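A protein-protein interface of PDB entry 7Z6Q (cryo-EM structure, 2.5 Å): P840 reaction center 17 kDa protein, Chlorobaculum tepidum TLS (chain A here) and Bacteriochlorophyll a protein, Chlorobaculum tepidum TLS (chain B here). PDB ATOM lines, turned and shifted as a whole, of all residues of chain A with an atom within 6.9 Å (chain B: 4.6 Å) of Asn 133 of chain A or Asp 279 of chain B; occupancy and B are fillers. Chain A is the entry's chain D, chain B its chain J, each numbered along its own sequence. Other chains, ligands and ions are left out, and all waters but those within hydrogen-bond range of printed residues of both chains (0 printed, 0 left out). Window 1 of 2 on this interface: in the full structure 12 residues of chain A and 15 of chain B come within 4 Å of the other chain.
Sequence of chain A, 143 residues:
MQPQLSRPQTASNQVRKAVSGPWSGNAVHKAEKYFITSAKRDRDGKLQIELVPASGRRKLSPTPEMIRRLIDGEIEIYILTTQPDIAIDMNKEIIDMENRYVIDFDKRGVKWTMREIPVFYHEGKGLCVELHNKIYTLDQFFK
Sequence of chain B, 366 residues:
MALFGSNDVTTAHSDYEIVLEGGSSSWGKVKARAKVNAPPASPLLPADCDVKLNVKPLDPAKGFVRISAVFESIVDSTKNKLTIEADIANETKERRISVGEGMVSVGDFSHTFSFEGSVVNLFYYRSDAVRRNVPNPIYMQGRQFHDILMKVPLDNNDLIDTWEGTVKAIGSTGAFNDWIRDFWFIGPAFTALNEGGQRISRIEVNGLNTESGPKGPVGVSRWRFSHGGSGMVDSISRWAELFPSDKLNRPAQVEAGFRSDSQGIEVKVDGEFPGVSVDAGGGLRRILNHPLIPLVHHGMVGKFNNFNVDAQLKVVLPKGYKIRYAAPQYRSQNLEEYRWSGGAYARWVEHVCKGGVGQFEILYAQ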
ATOM      1  N   GLU A  93       5.315  30.483   2.628  1.00  0.00           N
ATOM      2  CA  GLU A  93       6.133  29.701   1.659  1.00  0.00           C
ATOM      3  C   GLU A  93       6.919  28.615   2.407  1.00  0.00           C
ATOM      4  O   GLU A  93       6.932  27.456   1.929  1.00  0.00           O
ATOM      5  CB  GLU A  93       7.027  30.643   0.842  1.00  0.00           C
ATOM      6  CG  GLU A  93       7.857  29.958  -0.233  1.00  0.00           C
ATOM      7  CD  GLU A  93       8.716  30.873  -1.089  1.00  0.00           C
ATOM      8  OE1 GLU A  93       8.825  32.063  -0.750  1.00  0.00           O
ATOM      9  OE2 GLU A  93       9.284  30.388  -2.085  1.00  0.00           O
ATOM     10  N   ILE A 117      19.083  32.405   4.944  1.00  0.00           N
ATOM     11  CA  ILE A 117      19.166  32.548   3.459  1.00  0.00           C
ATOM     12  C   ILE A 117      20.544  33.109   3.113  1.00  0.00           C
ATOM     13  O   ILE A 117      20.871  34.199   3.600  1.00  0.00           O
ATOM     14  CB  ILE A 117      18.039  33.462   2.941  1.00  0.00           C
ATOM     15  CG1 ILE A 117      16.657  32.840   3.145  1.00  0.00           C
ATOM     16  CG2 ILE A 117      18.281  33.842   1.491  1.00  0.00           C
ATOM     17  CD1 ILE A 117      15.513  33.796   2.899  1.00  0.00           C
ATOM     18  N   PRO A 118      21.336  32.460   2.238  1.00  0.00           N
ATOM     19  CA  PRO A 118      22.665  32.959   1.930  1.00  0.00           C
ATOM     20  C   PRO A 118      22.625  34.105   0.914  1.00  0.00           C
ATOM     21  O   PRO A 118      22.376  33.865  -0.246  1.00  0.00           O
ATOM     22  CB  PRO A 118      23.345  31.750   1.277  1.00  0.00           C
ATOM     23  CG  PRO A 118      22.209  30.985   0.648  1.00  0.00           C
ATOM     24  CD  PRO A 118      21.011  31.224   1.543  1.00  0.00           C
ATOM     25  N   GLU A 130      18.685  34.550  -3.788  1.00  0.00           N
ATOM     26  CA  GLU A 130      18.080  33.563  -4.722  1.00  0.00           C
ATOM     27  C   GLU A 130      17.042  32.758  -3.931  1.00  0.00           C
ATOM     28  O   GLU A 130      17.343  31.604  -3.566  1.00  0.00           O
ATOM     29  CB  GLU A 130      19.162  32.656  -5.314  1.00  0.00           C
ATOM     30  CG  GLU A 130      18.642  31.720  -6.390  1.00  0.00           C
ATOM     31  CD  GLU A 130      19.574  30.572  -6.735  1.00  0.00           C
ATOM     32  OE1 GLU A 130      19.123  29.631  -7.418  1.00  0.00           O
ATOM     33  OE2 GLU A 130      20.748  30.622  -6.319  1.00  0.00           O
ATOM     34  N   LEU A 131      15.866  33.348  -3.684  1.00  0.00           N
ATOM     35  CA  LEU A 131      14.783  32.661  -2.937  1.00  0.00           C
ATOM     36  C   LEU A 131      13.815  31.989  -3.924  1.00  0.00           C
ATOM     37  O   LEU A 131      13.190  32.705  -4.727  1.00  0.00           O
ATOM     38  CB  LEU A 131      14.056  33.703  -2.079  1.00  0.00           C
ATOM     39  CG  LEU A 131      12.846  33.186  -1.307  1.00  0.00           C
ATOM     40  CD1 LEU A 131      12.859  33.696   0.125  1.00  0.00           C
ATOM     41  CD2 LEU A 131      11.555  33.578  -2.002  1.00  0.00           C
ATOM     42  N   HIS A 132      13.687  30.660  -3.824  1.00  0.00           N
ATOM     43  CA  HIS A 132      12.744  29.846  -4.641  1.00  0.00           C
ATOM     44  C   HIS A 132      12.960  30.039  -6.148  1.00  0.00           C
ATOM     45  O   HIS A 132      11.966  30.318  -6.847  1.00  0.00           O
ATOM     46  CB  HIS A 132      11.294  30.144  -4.232  1.00  0.00           C
ATOM     47  CG  HIS A 132      10.283  29.333  -4.970  1.00  0.00           C
ATOM     48  ND1 HIS A 132      10.317  27.952  -4.995  1.00  0.00           N
ATOM     49  CD2 HIS A 132       9.213  29.699  -5.708  1.00  0.00           C
ATOM     50  CE1 HIS A 132       9.312  27.502  -5.717  1.00  0.00           C
ATOM     51  NE2 HIS A 132       8.617  28.555  -6.167  1.00  0.00           N
ATOM     52  N   ASN A 133      14.203  29.903  -6.623  1.00  0.00           N
ATOM     53  CA  ASN A 133      14.526  30.019  -8.074  1.00  0.00           C
ATOM     54  C   ASN A 133      14.036  31.358  -8.643  1.00  0.00           C
ATOM     55  O   ASN A 133      13.486  31.354  -9.762  1.00  0.00           O
ATOM     56  CB  ASN A 133      13.978  28.835  -8.875  1.00  0.00           C
ATOM     57  CG  ASN A 133      14.817  28.506 -10.092  1.00  0.00           C
ATOM     58  OD1 ASN A 133      15.946  28.975 -10.219  1.00  0.00           O
ATOM     59  ND2 ASN A 133      14.276  27.700 -10.991  1.00  0.00           N
ATOM     60  N   LYS A 134      14.231  32.451  -7.900  1.00  0.00           N
ATOM     61  CA  LYS A 134      13.819  33.811  -8.338  1.00  0.00           C
ATOM     62  C   LYS A 134      14.756  34.814  -7.660  1.00  0.00           C
ATOM     63  O   LYS A 134      14.652  34.973  -6.427  1.00  0.00           O
ATOM     64  CB  LYS A 134      12.356  34.071  -7.967  1.00  0.00           C
ATOM     65  CG  LYS A 134      11.687  35.218  -8.713  1.00  0.00           C
ATOM     66  CD  LYS A 134      10.181  35.079  -8.794  1.00  0.00           C
ATOM     67  CE  LYS A 134       9.494  35.301  -7.464  1.00  0.00           C
ATOM     68  NZ  LYS A 134       8.019  35.348  -7.608  1.00  0.00           N
ATOM     69  N   ILE A 135      15.637  35.457  -8.432  1.00  0.00           N
ATOM     70  CA  ILE A 135      16.617  36.395  -7.812  1.00  0.00           C
ATOM     71  C   ILE A 135      15.868  37.615  -7.268  1.00  0.00           C
ATOM     72  O   ILE A 135      14.875  38.031  -7.880  1.00  0.00           O
ATOM     73  CB  ILE A 135      17.699  36.761  -8.847  1.00  0.00           C
ATOM     74  CG1 ILE A 135      18.434  35.512  -9.340  1.00  0.00           C
ATOM     75  CG2 ILE A 135      18.664  37.809  -8.321  1.00  0.00           C
ATOM     76  CD1 ILE A 135      19.795  35.787  -9.939  1.00  0.00           C
ATOM     77  N   SER B 277      22.349  23.450 -10.097  1.00  0.00           N
ATOM     78  CA  SER B 277      21.550  23.396  -8.844  1.00  0.00           C
ATOM     79  C   SER B 277      20.668  24.647  -8.738  1.00  0.00           C
ATOM     80  O   SER B 277      21.197  25.761  -8.924  1.00  0.00           O
ATOM     81  CB  SER B 277      22.444  23.252  -7.640  1.00  0.00           C
ATOM     82  OG  SER B 277      23.377  24.321  -7.572  1.00  0.00           O
ATOM     83  N   VAL B 278      19.376  24.458  -8.452  1.00  0.00           N
ATOM     84  CA  VAL B 278      18.419  25.600  -8.328  1.00  0.00           C
ATOM     85  C   VAL B 278      17.625  25.446  -7.025  1.00  0.00           C
ATOM     86  O   VAL B 278      17.394  24.296  -6.605  1.00  0.00           O
ATOM     87  CB  VAL B 278      17.484  25.685  -9.550  1.00  0.00           C
ATOM     88  CG1 VAL B 278      18.251  25.976 -10.829  1.00  0.00           C
ATOM     89  CG2 VAL B 278      16.640  24.427  -9.704  1.00  0.00           C
ATOM     90  N   ASP B 279      17.224  26.570  -6.422  1.00  0.00           N
ATOM     91  CA  ASP B 279      16.446  26.562  -5.153  1.00  0.00           C
ATOM     92  C   ASP B 279      15.118  25.831  -5.380  1.00  0.00           C
ATOM     93  O   ASP B 279      14.510  26.027  -6.452  1.00  0.00           O
ATOM     94  CB  ASP B 279      16.232  27.982  -4.622  1.00  0.00           C
ATOM     95  CG  ASP B 279      15.872  28.027  -3.148  1.00  0.00           C
ATOM     96  OD1 ASP B 279      14.896  27.353  -2.763  1.00  0.00           O
ATOM     97  OD2 ASP B 279      16.570  28.735  -2.395  1.00  0.00           O
ATOM     98  N   ALA B 280      14.688  25.030  -4.400  1.00  0.00           N
ATOM     99  CA  ALA B 280      13.448  24.279  -4.509  1.00  0.00           C
ATOM    100  C   ALA B 280      12.410  24.684  -3.469  1.00  0.00           C
ATOM    101  O   ALA B 280      11.299  24.142  -3.488  1.00  0.00           O
ATOM    102  CB  ALA B 280      13.724  22.775  -4.392  1.00  0.00           C
ATOM    103  N   GLY B 281      12.734  25.605  -2.573  1.00  0.00           N
ATOM    104  CA  GLY B 281      11.795  26.052  -1.554  1.00  0.00           C
ATOM    105  C   GLY B 281      12.019  25.377  -0.218  1.00  0.00           C
ATOM    106  O   GLY B 281      12.445  24.226  -0.127  1.00  0.00           O
ATOM    107  N   LEU B 284      15.589  24.114   0.732  1.00  0.00           N
ATOM    108  CA  LEU B 284      16.112  22.894   0.059  1.00  0.00           C
ATOM    109  C   LEU B 284      16.585  23.197  -1.367  1.00  0.00           C
ATOM    110  O   LEU B 284      15.892  23.944  -2.084  1.00  0.00           O
ATOM    111  CB  LEU B 284      15.015  21.824   0.055  1.00  0.00           C
ATOM    112  CG  LEU B 284      14.928  20.969   1.318  1.00  0.00           C
ATOM    113  CD1 LEU B 284      14.591  21.825   2.530  1.00  0.00           C
ATOM    114  CD2 LEU B 284      13.905  19.856   1.152  1.00  0.00           C
ATOM    115  N   ARG B 285      17.734  22.622  -1.739  1.00  0.00           N
ATOM    116  CA  ARG B 285      18.304  22.758  -3.106  1.00  0.00           C
ATOM    117  C   ARG B 285      17.873  21.537  -3.930  1.00  0.00           C
ATOM    118  O   ARG B 285      17.395  20.552  -3.326  1.00  0.00           O
ATOM    119  CB  ARG B 285      19.832  22.867  -3.040  1.00  0.00           C
ATOM    120  CG  ARG B 285      20.339  24.210  -2.535  1.00  0.00           C
ATOM    121  CD  ARG B 285      21.670  24.593  -3.155  1.00  0.00           C
ATOM    122  NE  ARG B 285      21.550  24.918  -4.568  1.00  0.00           N
ATOM    123  CZ  ARG B 285      21.243  26.121  -5.040  1.00  0.00           C
ATOM    124  NH1 ARG B 285      20.823  27.067  -4.219  1.00  0.00           N
ATOM    125  NH2 ARG B 285      21.356  26.371  -6.333  1.00  0.00           N
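The backbone carbonyl oxygen (O) of Glu 130 of chain A lies close to the side-chain carboxylate (OD2) of Asp 279 of chain B (3.2 Å).
The side-chain carboxylate (OD1) of Asp 279 of chain B lies within hydrogen-bond range of the backbone NH (N) of Gly 281 of chain B (2.8 Å).
Among the printed residues, merely in contact across the chains: His 132 of chain A with Asp 279 of chain B (3.5 Å), Asn 133 of chain A with Val 278 of chain B (3.7 Å) and Asn 133 of chain A with Asp 279 of chain B (3.4 Å).
Glu 93 of chain A touches none of the printed residues of chain B. Of the printed residues of chain B, Glu 130 of chain A touches Asp 279. Leu 131 of chain A touches none of the printed residues of chain B. Printed residues of chain B within 4 Å of His 132 of chain A: Asp 279. Asn 133 of chain A touches just these residues of chain B: Val 278 (3.7 Å) and Asp 279 (3.4 Å). Printed residues of chain A within 4 Å of Val 278 of chain B: Asn 133 (3.7 Å). Asp 279 of chain B touches just these residues of chain A: Glu 130, His 132 and Asn 133. The nearest printed residue of chain B that does not touch Asn 133 of chain A is Ala 280 of chain B (5.4 Å).
Printed residues of chain A that touch a printed residue of chain B: Glu 130, His 132 and Asn 133. Of the 7 printed residues of chain B, 2 touch a printed residue of chain A.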
